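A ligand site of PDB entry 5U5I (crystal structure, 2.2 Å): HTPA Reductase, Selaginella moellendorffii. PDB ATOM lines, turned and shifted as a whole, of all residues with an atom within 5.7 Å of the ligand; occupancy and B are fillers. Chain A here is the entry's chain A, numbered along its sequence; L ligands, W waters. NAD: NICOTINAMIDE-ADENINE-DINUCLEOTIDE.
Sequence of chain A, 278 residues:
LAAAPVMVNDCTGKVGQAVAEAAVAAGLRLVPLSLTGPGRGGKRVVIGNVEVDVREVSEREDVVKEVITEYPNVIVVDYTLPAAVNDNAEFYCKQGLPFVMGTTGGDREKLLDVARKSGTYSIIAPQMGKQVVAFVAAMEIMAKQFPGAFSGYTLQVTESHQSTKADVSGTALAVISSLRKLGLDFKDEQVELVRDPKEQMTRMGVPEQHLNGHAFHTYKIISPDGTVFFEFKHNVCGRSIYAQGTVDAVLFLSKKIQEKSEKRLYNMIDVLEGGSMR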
ATOM      1  N   ASN A   9       6.652  13.921   9.090  1.00  0.00           N
ATOM      2  CA  ASN A   9       7.232  14.780   8.060  1.00  0.00           C
ATOM      3  C   ASN A   9       7.513  16.129   8.718  1.00  0.00           C
ATOM      4  O   ASN A   9       6.561  16.812   9.078  1.00  0.00           O
ATOM      5  CB  ASN A   9       6.230  14.968   6.910  1.00  0.00           C
ATOM      6  CG  ASN A   9       5.867  13.668   6.222  1.00  0.00           C
ATOM      7  OD1 ASN A   9       6.674  12.731   6.179  1.00  0.00           O
ATOM      8  ND2 ASN A   9       4.656  13.606   5.674  1.00  0.00           N
ATOM      9  N   ASP A  10       8.767  16.585   8.875  1.00  0.00           N
ATOM     10  CA  ASP A  10      10.018  16.032   8.352  1.00  0.00           C
ATOM     11  C   ASP A  10      10.870  15.476   9.513  1.00  0.00           C
ATOM     12  O   ASP A  10      11.201  16.222  10.444  1.00  0.00           O
ATOM     13  CB  ASP A  10      10.747  17.198   7.642  1.00  0.00           C
ATOM     14  CG  ASP A  10      12.154  16.835   7.095  1.00  0.00           C
ATOM     15  OD1 ASP A  10      12.651  15.696   7.261  1.00  0.00           O
ATOM     16  OD2 ASP A  10      12.792  17.745   6.498  1.00  0.00           O
ATOM     17  N   THR A  12      13.917  14.786   9.557  1.00  0.00           N
ATOM     18  CA  THR A  12      15.219  15.462   9.571  1.00  0.00           C
ATOM     19  C   THR A  12      15.183  16.931  10.058  1.00  0.00           C
ATOM     20  O   THR A  12      16.226  17.497  10.351  1.00  0.00           O
ATOM     21  CB  THR A  12      15.916  15.410   8.191  1.00  0.00           C
ATOM     22  OG1 THR A  12      15.214  16.214   7.231  1.00  0.00           O
ATOM     23  CG2 THR A  12      15.977  13.985   7.707  1.00  0.00           C
ATOM     24  N   GLY A  13      14.000  17.536  10.136  1.00  0.00           N
ATOM     25  CA  GLY A  13      13.839  18.813  10.835  1.00  0.00           C
ATOM     26  C   GLY A  13      14.075  18.665  12.337  1.00  0.00           C
ATOM     27  O   GLY A  13      14.057  17.552  12.869  1.00  0.00           O
ATOM     28  N   LYS A  14      14.313  19.764  13.038  1.00  0.00           N
ATOM     29  CA  LYS A  14      14.712  19.684  14.446  1.00  0.00           C
ATOM     30  C   LYS A  14      13.564  19.202  15.330  1.00  0.00           C
ATOM     31  O   LYS A  14      13.750  18.284  16.125  1.00  0.00           O
ATOM     32  CB  LYS A  14      15.307  21.012  14.928  1.00  0.00           C
ATOM     33  CG  LYS A  14      16.635  21.329  14.261  1.00  0.00           C
ATOM     34  CD  LYS A  14      17.395  22.499  14.871  1.00  0.00           C
ATOM     35  CE  LYS A  14      16.646  23.811  14.760  1.00  0.00           C
ATOM     36  NZ  LYS A  14      16.199  24.130  13.377  1.00  0.00           N
ATOM     37  N   VAL A  15      12.356  19.738  15.144  1.00  0.00           N
ATOM     38  CA  VAL A  15      11.216  19.300  15.964  1.00  0.00           C
ATOM     39  C   VAL A  15      10.712  17.943  15.481  1.00  0.00           C
ATOM     40  O   VAL A  15      10.460  17.037  16.289  1.00  0.00           O
ATOM     41  CB  VAL A  15      10.054  20.322  15.998  1.00  0.00           C
ATOM     42  CG1 VAL A  15       8.932  19.821  16.902  1.00  0.00           C
ATOM     43  CG2 VAL A  15      10.530  21.690  16.482  1.00  0.00           C
ATOM     44  N   GLY A  16      10.589  17.792  14.168  1.00  0.00           N
ATOM     45  CA  GLY A  16      10.192  16.532  13.581  1.00  0.00           C
ATOM     46  C   GLY A  16      11.066  15.378  13.978  1.00  0.00           C
ATOM     47  O   GLY A  16      10.560  14.294  14.243  1.00  0.00           O
ATOM     48  N   LEU A  35       8.943  12.713   4.349  1.00  0.00           N
ATOM     49  CA  LEU A  35       9.106  13.757   3.333  1.00  0.00           C
ATOM     50  C   LEU A  35       9.915  14.917   3.906  1.00  0.00           C
ATOM     51  O   LEU A  35       9.683  15.347   5.043  1.00  0.00           O
ATOM     52  CB  LEU A  35       7.744  14.254   2.852  1.00  0.00           C
ATOM     53  CG  LEU A  35       6.813  13.219   2.219  1.00  0.00           C
ATOM     54  CD1 LEU A  35       5.449  13.834   1.926  1.00  0.00           C
ATOM     55  CD2 LEU A  35       7.420  12.615   0.950  1.00  0.00           C
ATOM     56  N   THR A  36      10.855  15.410   3.105  1.00  0.00           N
ATOM     57  CA  THR A  36      11.690  16.541   3.500  1.00  0.00           C
ATOM     58  C   THR A  36      11.411  17.689   2.519  1.00  0.00           C
ATOM     59  O   THR A  36      10.653  17.512   1.561  1.00  0.00           O
ATOM     60  CB  THR A  36      13.177  16.126   3.570  1.00  0.00           C
ATOM     61  OG1 THR A  36      13.975  17.200   4.075  1.00  0.00           O
ATOM     62  CG2 THR A  36      13.708  15.667   2.201  1.00  0.00           C
ATOM     63  N   GLY A  37      12.000  18.865   2.772  1.00  0.00           N
ATOM     64  CA  GLY A  37      11.583  20.098   2.087  1.00  0.00           C
ATOM     65  C   GLY A  37      12.275  20.351   0.751  1.00  0.00           C
ATOM     66  O   GLY A  37      13.212  19.629   0.390  1.00  0.00           O
ATOM     67  N   PRO A  38      11.821  21.395   0.020  1.00  0.00           N
ATOM     68  CA  PRO A  38      12.430  21.770  -1.259  1.00  0.00           C
ATOM     69  C   PRO A  38      13.942  22.019  -1.119  1.00  0.00           C
ATOM     70  O   PRO A  38      14.372  22.658  -0.159  1.00  0.00           O
ATOM     71  CB  PRO A  38      11.707  23.055  -1.643  1.00  0.00           C
ATOM     72  CG  PRO A  38      10.416  23.026  -0.887  1.00  0.00           C
ATOM     73  CD  PRO A  38      10.745  22.338   0.391  1.00  0.00           C
ATOM     74  N   ARG A  40      16.240  19.978  -0.218  1.00  0.00           N
ATOM     75  CA  ARG A  40      16.840  18.862   0.512  1.00  0.00           C
ATOM     76  C   ARG A  40      16.722  17.629  -0.370  1.00  0.00           C
ATOM     77  O   ARG A  40      15.717  17.437  -1.044  1.00  0.00           O
ATOM     78  CB  ARG A  40      16.133  18.624   1.842  1.00  0.00           C
ATOM     79  CG  ARG A  40      16.100  19.830   2.786  1.00  0.00           C
ATOM     80  CD  ARG A  40      17.481  20.345   3.175  1.00  0.00           C
ATOM     81  NE  ARG A  40      18.327  19.318   3.803  1.00  0.00           N
ATOM     82  CZ  ARG A  40      19.631  19.426   4.040  1.00  0.00           C
ATOM     83  NH1 ARG A  40      20.300  20.538   3.747  1.00  0.00           N
ATOM     84  NH2 ARG A  40      20.281  18.416   4.606  1.00  0.00           N
ATOM     85  N   VAL A  57      10.061  16.023  -1.370  1.00  0.00           N
ATOM     86  CA  VAL A  57       8.611  16.316  -1.364  1.00  0.00           C
ATOM     87  C   VAL A  57       7.919  16.153  -2.733  1.00  0.00           C
ATOM     88  O   VAL A  57       6.740  15.840  -2.776  1.00  0.00           O
ATOM     89  CB  VAL A  57       8.330  17.727  -0.788  1.00  0.00           C
ATOM     90  CG1 VAL A  57       8.750  18.814  -1.783  1.00  0.00           C
ATOM     91  CG2 VAL A  57       6.860  17.867  -0.386  1.00  0.00           C
ATOM     92  N   TYR A  79       5.626  18.666  11.083  1.00  0.00           N
ATOM     93  CA  TYR A  79       6.494  19.768  11.533  1.00  0.00           C
ATOM     94  C   TYR A  79       7.411  20.172  10.366  1.00  0.00           C
ATOM     95  O   TYR A  79       8.554  19.697  10.253  1.00  0.00           O
ATOM     96  CB  TYR A  79       7.317  19.344  12.746  1.00  0.00           C
ATOM     97  CG  TYR A  79       6.517  19.362  14.013  1.00  0.00           C
ATOM     98  CD1 TYR A  79       6.398  20.532  14.746  1.00  0.00           C
ATOM     99  CD2 TYR A  79       5.884  18.217  14.488  1.00  0.00           C
ATOM    100  CE1 TYR A  79       5.670  20.570  15.917  1.00  0.00           C
ATOM    101  CE2 TYR A  79       5.149  18.243  15.669  1.00  0.00           C
ATOM    102  CZ  TYR A  79       5.052  19.427  16.375  1.00  0.00           C
ATOM    103  OH  TYR A  79       4.329  19.487  17.536  1.00  0.00           O
ATOM    104  N   THR A  80       6.891  21.039   9.506  1.00  0.00           N
ATOM    105  CA  THR A  80       7.603  21.531   8.321  1.00  0.00           C
ATOM    106  C   THR A  80       7.845  23.051   8.426  1.00  0.00           C
ATOM    107  O   THR A  80       8.530  23.477   9.348  1.00  0.00           O
ATOM    108  CB  THR A  80       6.845  21.118   7.040  1.00  0.00           C
ATOM    109  OG1 THR A  80       5.509  21.624   7.101  1.00  0.00           O
ATOM    110  CG2 THR A  80       6.806  19.603   6.932  1.00  0.00           C
ATOM    111  N   LEU A  81       7.325  23.859   7.499  1.00  0.00           N
ATOM    112  CA  LEU A  81       7.571  25.297   7.519  1.00  0.00           C
ATOM    113  C   LEU A  81       6.271  26.025   7.171  1.00  0.00           C
ATOM    114  O   LEU A  81       5.412  25.425   6.528  1.00  0.00           O
ATOM    115  CB  LEU A  81       8.672  25.670   6.525  1.00  0.00           C
ATOM    116  CG  LEU A  81      10.112  25.185   6.818  1.00  0.00           C
ATOM    117  CD1 LEU A  81      11.048  25.498   5.655  1.00  0.00           C
ATOM    118  CD2 LEU A  81      10.669  25.782   8.105  1.00  0.00           C
ATOM    119  N   PRO A  82       6.119  27.304   7.611  1.00  0.00           N
ATOM    120  CA  PRO A  82       4.899  28.068   7.326  1.00  0.00           C
ATOM    121  C   PRO A  82       4.465  28.042   5.854  1.00  0.00           C
ATOM    122  O   PRO A  82       3.263  27.978   5.581  1.00  0.00           O
ATOM    123  CB  PRO A  82       5.260  29.497   7.749  1.00  0.00           C
ATOM    124  CG  PRO A  82       6.327  29.339   8.768  1.00  0.00           C
ATOM    125  CD  PRO A  82       7.077  28.081   8.424  1.00  0.00           C
ATOM    126  N   ALA A  84       4.709  25.654   3.755  1.00  0.00           N
ATOM    127  CA  ALA A  84       4.141  24.342   3.395  1.00  0.00           C
ATOM    128  C   ALA A  84       2.777  24.026   4.030  1.00  0.00           C
ATOM    129  O   ALA A  84       2.085  23.106   3.584  1.00  0.00           O
ATOM    130  CB  ALA A  84       5.126  23.244   3.745  1.00  0.00           C
ATOM    131  N   ASN A  88       0.301  21.303   2.284  1.00  0.00           N
ATOM    132  CA  ASN A  88       0.321  20.019   3.022  1.00  0.00           C
ATOM    133  C   ASN A  88      -1.053  19.602   3.570  1.00  0.00           C
ATOM    134  O   ASN A  88      -1.448  18.438   3.415  1.00  0.00           O
ATOM    135  CB  ASN A  88       1.288  20.078   4.211  1.00  0.00           C
ATOM    136  CG  ASN A  88       2.733  20.032   3.782  1.00  0.00           C
ATOM    137  OD1 ASN A  88       3.057  19.924   2.589  1.00  0.00           O
ATOM    138  ND2 ASN A  88       3.616  20.121   4.764  1.00  0.00           N
ATOM    139  N   MET A 101      -0.999  18.598  13.062  1.00  0.00           N
ATOM    140  CA  MET A 101      -0.274  19.747  12.489  1.00  0.00           C
ATOM    141  C   MET A 101       0.308  20.589  13.591  1.00  0.00           C
ATOM    142  O   MET A 101      -0.404  21.338  14.259  1.00  0.00           O
ATOM    143  CB  MET A 101      -1.242  20.524  11.597  1.00  0.00           C
ATOM    144  CG  MET A 101      -0.822  21.912  11.118  1.00  0.00           C
ATOM    145  SD  MET A 101       0.416  21.819   9.603  1.00  0.00           S
ATOM    146  CE  MET A 101      -0.666  20.981   8.191  1.00  0.00           C
ATOM    147  N   GLY A 102       1.632  20.471  13.761  1.00  0.00           N
ATOM    148  CA  GLY A 102       2.403  21.312  14.659  1.00  0.00           C
ATOM    149  C   GLY A 102       2.982  22.579  14.041  1.00  0.00           C
ATOM    150  O   GLY A 102       3.195  23.567  14.734  1.00  0.00           O
ATOM    151  N   THR A 103       3.219  22.554  12.730  1.00  0.00           N
ATOM    152  CA  THR A 103       3.833  23.696  12.029  1.00  0.00           C
ATOM    153  C   THR A 103       3.044  24.993  12.274  1.00  0.00           C
ATOM    154  O   THR A 103       1.804  24.992  12.256  1.00  0.00           O
ATOM    155  CB  THR A 103       3.949  23.380  10.521  1.00  0.00           C
ATOM    156  OG1 THR A 103       4.481  22.060  10.347  1.00  0.00           O
ATOM    157  CG2 THR A 103       4.850  24.381   9.795  1.00  0.00           C
ATOM    158  N   THR A 104       3.755  26.084  12.563  1.00  0.00           N
ATOM    159  CA  THR A 104       3.134  27.391  12.795  1.00  0.00           C
ATOM    160  C   THR A 104       3.117  28.216  11.514  1.00  0.00           C
ATOM    161  O   THR A 104       3.830  27.906  10.533  1.00  0.00           O
ATOM    162  CB  THR A 104       3.873  28.195  13.885  1.00  0.00           C
ATOM    163  OG1 THR A 104       5.252  28.348  13.532  1.00  0.00           O
ATOM    164  CG2 THR A 104       3.778  27.496  15.246  1.00  0.00           C
ATOM    165  N   GLY A 105       2.283  29.255  11.519  1.00  0.00           N
ATOM    166  CA  GLY A 105       2.166  30.161  10.390  1.00  0.00           C
ATOM    167  C   GLY A 105       1.310  29.601   9.272  1.00  0.00           C
ATOM    168  O   GLY A 105       0.540  28.652   9.487  1.00  0.00           O
ATOM    169  N   ALA A 125      -2.745  22.445  16.214  1.00  0.00           N
ATOM    170  CA  ALA A 125      -2.364  23.134  17.448  1.00  0.00           C
ATOM    171  C   ALA A 125      -0.996  23.772  17.318  1.00  0.00           C
ATOM    172  O   ALA A 125       0.023  23.092  17.398  1.00  0.00           O
ATOM    173  CB  ALA A 125      -2.386  22.161  18.626  1.00  0.00           C
ATOM    174  N   PRO A 126      -0.956  25.120  17.159  1.00  0.00           N
ATOM    175  CA  PRO A 126       0.334  25.809  17.105  1.00  0.00           C
ATOM    176  C   PRO A 126       1.107  25.842  18.437  1.00  0.00           C
ATOM    177  O   PRO A 126       2.294  26.161  18.440  1.00  0.00           O
ATOM    178  CB  PRO A 126      -0.040  27.233  16.655  1.00  0.00           C
ATOM    179  CG  PRO A 126      -1.468  27.410  17.046  1.00  0.00           C
ATOM    180  CD  PRO A 126      -2.086  26.060  17.262  1.00  0.00           C
ATOM    181  N   GLN A 127       0.443  25.508  19.548  1.00  0.00           N
ATOM    182  CA  GLN A 127       1.125  25.274  20.837  1.00  0.00           C
ATOM    183  C   GLN A 127       0.845  23.832  21.310  1.00  0.00           C
ATOM    184  O   GLN A 127      -0.267  23.527  21.780  1.00  0.00           O
ATOM    185  CB  GLN A 127       0.692  26.347  21.861  1.00  0.00           C
ATOM    186  CG  GLN A 127       1.121  26.147  23.322  1.00  0.00           C
ATOM    187  CD  GLN A 127       2.621  26.133  23.588  1.00  0.00           C
ATOM    188  OE1 GLN A 127       3.305  25.199  23.182  1.00  0.00           O
ATOM    189  NE2 GLN A 127       3.131  27.117  24.319  1.00  0.00           N
ATOM    190  N   MET A 128       1.863  22.974  21.186  1.00  0.00           N
ATOM    191  CA  MET A 128       1.799  21.570  21.585  1.00  0.00           C
ATOM    192  C   MET A 128       2.395  21.285  22.947  1.00  0.00           C
ATOM    193  O   MET A 128       2.326  20.147  23.413  1.00  0.00           O
ATOM    194  CB  MET A 128       2.528  20.754  20.531  1.00  0.00           C
ATOM    195  CG  MET A 128       2.027  19.311  20.455  1.00  0.00           C
ATOM    196  SD  MET A 128       0.529  19.119  19.192  1.00  0.00           S
ATOM    197  CE  MET A 128       1.187  19.683  17.427  1.00  0.00           C
ATOM    198  N   GLY A 129       2.959  22.287  23.609  1.00  0.00           N
ATOM    199  CA  GLY A 129       3.466  22.121  24.974  1.00  0.00           C
ATOM    200  C   GLY A 129       2.337  22.000  25.966  1.00  0.00           C
ATOM    201  O   GLY A 129       2.001  22.974  26.663  1.00  0.00           O
ATOM    202  N   ARG A 239      12.954  20.944  23.256  1.00  0.00           N
ATOM    203  CA  ARG A 239      11.815  20.502  22.451  1.00  0.00           C
ATOM    204  C   ARG A 239      10.977  19.337  23.012  1.00  0.00           C
ATOM    205  O   ARG A 239       9.910  19.037  22.467  1.00  0.00           O
ATOM    206  CB  ARG A 239      12.329  20.120  21.059  1.00  0.00           C
ATOM    207  CG  ARG A 239      12.998  21.286  20.362  1.00  0.00           C
ATOM    208  CD  ARG A 239      13.532  20.926  18.984  1.00  0.00           C
ATOM    209  NE  ARG A 239      14.525  21.928  18.601  1.00  0.00           N
ATOM    210  CZ  ARG A 239      15.854  21.780  18.671  1.00  0.00           C
ATOM    211  NH1 ARG A 239      16.416  20.647  19.097  1.00  0.00           N
ATOM    212  NH2 ARG A 239      16.635  22.797  18.295  1.00  0.00           N
ATOM    213  N   TYR A 242       7.213  19.535  23.513  1.00  0.00           N
ATOM    214  CA  TYR A 242       6.479  19.531  22.242  1.00  0.00           C
ATOM    215  C   TYR A 242       6.449  18.128  21.675  1.00  0.00           C
ATOM    216  O   TYR A 242       5.430  17.709  21.155  1.00  0.00           O
ATOM    217  CB  TYR A 242       7.094  20.520  21.242  1.00  0.00           C
ATOM    218  CG  TYR A 242       7.224  21.883  21.842  1.00  0.00           C
ATOM    219  CD1 TYR A 242       6.082  22.657  22.115  1.00  0.00           C
ATOM    220  CD2 TYR A 242       8.463  22.393  22.221  1.00  0.00           C
ATOM    221  CE1 TYR A 242       6.199  23.904  22.712  1.00  0.00           C
ATOM    222  CE2 TYR A 242       8.584  23.631  22.820  1.00  0.00           C
ATOM    223  CZ  TYR A 242       7.449  24.388  23.054  1.00  0.00           C
ATOM    224  OH  TYR A 242       7.557  25.631  23.650  1.00  0.00           O
HETATM  225  PA  NAD L   1      13.378  23.145  10.898  1.00  0.00           P
HETATM  226  O1A NAD L   1      13.774  24.204   9.919  1.00  0.00           O
HETATM  227  O2A NAD L   1      14.404  22.542  11.822  1.00  0.00           O
HETATM  228  O5B NAD L   1      12.681  21.923  10.133  1.00  0.00           O
HETATM  229  C5B NAD L   1      11.661  22.122   9.166  1.00  0.00           C
HETATM  230  C4B NAD L   1      11.815  21.022   8.132  1.00  0.00           C
HETATM  231  O4B NAD L   1      10.699  21.014   7.250  1.00  0.00           O
HETATM  232  C3B NAD L   1      13.054  21.194   7.274  1.00  0.00           C
HETATM  233  O3B NAD L   1      13.874  20.029   7.371  1.00  0.00           O
HETATM  234  C2B NAD L   1      12.515  21.383   5.865  1.00  0.00           C
HETATM  235  O2B NAD L   1      13.361  20.824   4.863  1.00  0.00           O
HETATM  236  C1B NAD L   1      11.173  20.667   5.948  1.00  0.00           C
HETATM  237  N9A NAD L   1      10.159  21.025   4.935  1.00  0.00           N
HETATM  238  C8A NAD L   1       9.946  22.236   4.376  1.00  0.00           C
HETATM  239  N7A NAD L   1       8.906  22.183   3.501  1.00  0.00           N
HETATM  240  C5A NAD L   1       8.446  20.920   3.515  1.00  0.00           C
HETATM  241  C6A NAD L   1       7.373  20.177   2.821  1.00  0.00           C
HETATM  242  N6A NAD L   1       6.590  20.821   1.935  1.00  0.00           N
HETATM  243  N1A NAD L   1       7.207  18.862   3.107  1.00  0.00           N
HETATM  244  C2A NAD L   1       8.002  18.221   3.986  1.00  0.00           C
HETATM  245  N3A NAD L   1       9.009  18.853   4.649  1.00  0.00           N
HETATM  246  C4A NAD L   1       9.268  20.161   4.455  1.00  0.00           C
HETATM  247  O3  NAD L   1      12.123  23.753  11.730  1.00  0.00           O
HETATM  248  PN  NAD L   1      11.760  23.308  13.236  1.00  0.00           P
HETATM  249  O1N NAD L   1      12.691  24.071  14.137  1.00  0.00           O
HETATM  250  O2N NAD L   1      11.644  21.810  13.303  1.00  0.00           O
HETATM  251  O5D NAD L   1      10.274  23.900  13.370  1.00  0.00           O
HETATM  252  C5D NAD L   1       9.253  23.368  12.535  1.00  0.00           C
HETATM  253  C4D NAD L   1       7.948  24.141  12.654  1.00  0.00           C
HETATM  254  O4D NAD L   1       7.297  23.791  13.875  1.00  0.00           O
HETATM  255  C3D NAD L   1       8.131  25.655  12.689  1.00  0.00           C
HETATM  256  O3D NAD L   1       7.038  26.257  11.986  1.00  0.00           O
HETATM  257  C2D NAD L   1       8.097  26.001  14.178  1.00  0.00           C
HETATM  258  O2D NAD L   1       7.679  27.350  14.425  1.00  0.00           O
HETATM  259  C1D NAD L   1       7.078  24.976  14.660  1.00  0.00           C
HETATM  260  N1N NAD L   1       7.084  24.585  16.085  1.00  0.00           N
HETATM  261  C2N NAD L   1       5.880  24.322  16.617  1.00  0.00           C
HETATM  262  C3N NAD L   1       5.733  23.925  17.943  1.00  0.00           C
HETATM  263  C7N NAD L   1       4.365  23.642  18.532  1.00  0.00           C
HETATM  264  O7N NAD L   1       4.224  23.663  19.746  1.00  0.00           O
HETATM  265  N7N NAD L   1       3.301  23.360  17.765  1.00  0.00           N
HETATM  266  C4N NAD L   1       6.895  23.796  18.716  1.00  0.00           C
HETATM  267  C5N NAD L   1       8.135  24.054  18.143  1.00  0.00           C
HETATM  268  C6N NAD L   1       8.212  24.455  16.816  1.00  0.00           C
HETATM  269  O   HOH W   1      14.983  23.033   4.743  1.00  0.00           O
HETATM  270  O   HOH W   2      13.816  26.391  13.289  1.00  0.00           O
HETATM  271  O   HOH W   3      10.788  19.632  11.890  1.00  0.00           O
HETATM  272  O   HOH W   4      16.702  22.105  10.188  1.00  0.00           O
HETATM  273  O   HOH W   5       8.081  28.664  11.735  1.00  0.00           O
HETATM  274  O   HOH W   6      14.418  24.561   7.436  1.00  0.00           O
HETATM  275  O   HOH W   7      12.813  27.019  10.827  1.00  0.00           O
HETATM  276  O   HOH W   8      13.226  22.979   2.832  1.00  0.00           O
HETATM  277  O   HOH W   9       4.725  26.731  20.453  1.00  0.00           O
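The side-chain amino group (NZ) of Lys 14 is in salt-bridge range of an oxygen (O2A) of the ligand, 2.9 Å away.
The backbone NH of Lys 14 lies within hydrogen-bond range of an oxygen (O2A) of the ligand (3.0 Å).
The backbone carbonyl oxygen of Gly 102 sits at hydrogen-bond distance from a nitrogen (N7N) of the ligand (3.0 Å).
O2N of the ligand sits at hydrogen-bond distance from N of Val 15 (2.9 Å).
N of Met 128 sits at hydrogen-bond distance from O7N of the ligand.
A nitrogen (N7N) of the ligand sits at hydrogen-bond distance from the backbone carbonyl oxygen (O) of Pro 126.
The backbone NH of Thr 104 lies within hydrogen-bond range of an oxygen (O3D) of the ligand (3.3 Å).
OG1 of Thr 104 is in hydrogen-bond range of O2D of the ligand (2.8 Å).
N of Gly 37 is in hydrogen-bond range of O2B of the ligand (3.2 Å).
An oxygen (O3B) of the ligand lies within hydrogen-bond range of the side-chain carboxylate (OD2) of Asp 10 (2.7 Å).
N7N of the ligand is in hydrogen-bond range of O of Ala 125 (3.3 Å).
O of Thr 36 sits close to N of Val 57 (3.3 Å).
The backbone carbonyl oxygen (O) of Ala 84 sits close to the side-chain amide oxygen (OD1) of Asn 88, at 3.5 Å.
O of Tyr 79 lies within hydrogen-bond range of N of Asp 10, 3.4 Å away.
The side-chain carboxylate (OD1) of Asp 10 is in hydrogen-bond range of the side-chain hydroxyl (OG1) of Thr 12.
The side-chain amide oxygen (OE1) of Gln 127 sits at hydrogen-bond distance from the backbone NH (N) of Gly 129 (3.0 Å).
The side-chain hydroxyl of Thr 80 is in hydrogen-bond range of the side-chain amide nitrogen of Asn 88 (3.4 Å).
The backbone carbonyl oxygen (O) of Met 101 sits at hydrogen-bond distance from the backbone NH (N) of Ala 125 (3.2 Å).
N of Thr 80 sits at hydrogen-bond distance from OG1 of Thr 103, 2.7 Å away.
Gly 13 touches the ligand (CA to O5B, 3.4 Å).
Leu 35 touches the ligand (O to C2A, 3.5 Å).
C of Thr 36 touches N3A of the ligand, 3.4 Å away.
CD of Pro 38 touches N7A of the ligand (3.6 Å).
Arg 40 touches the ligand (CG to O2B, 3.6 Å).
CG2 of Val 57 touches N1A of the ligand, 3.6 Å away.
Tyr 79 touches the ligand (CD1 to O4D, 3.5 Å).
Thr 80 touches the ligand.
CD1 of Leu 81 touches C8A of the ligand, at 3.7 Å.
Ala 84 touches the ligand (CB to N6A, 3.4 Å).
Asn 88 touches the ligand (OD1 to N6A, 3.7 Å).
CG2 of Thr 103 touches O3D of the ligand, at 3.6 Å.
Gln 127 touches the ligand (CA to O7N, 3.7 Å).
Tyr 242 touches the ligand (CD1 to O7N, 3.2 Å).
Within 4 Å of the ligand: Asp 10, Gly 13, Lys 14, Val 15, Leu 35, Thr 36, Gly 37, Pro 38, Arg 40, Val 57, Tyr 79, Thr 80, Leu 81, Ala 84, Asn 88, Gly 102, Thr 103, Thr 104, Ala 125, Pro 126, Gln 127, Met 128 and Tyr 242.
Water W5 bridges O3D of the ligand and OG1 of Thr 104.
Water W2 bridges O1N of the ligand (2.7 Å) and NZ of Lys 14 (3.3 Å).
Water W3 lies within hydrogen-bond range of an oxygen (O2N) of the ligand (2.7 Å), the backbone carbonyl oxygen (O) of Tyr 79 (2.8 Å) and the backbone NH (N) of Gly 16 (2.9 Å).
Water W8 lies within hydrogen-bond range of O2B of the ligand and O of Pro 38.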
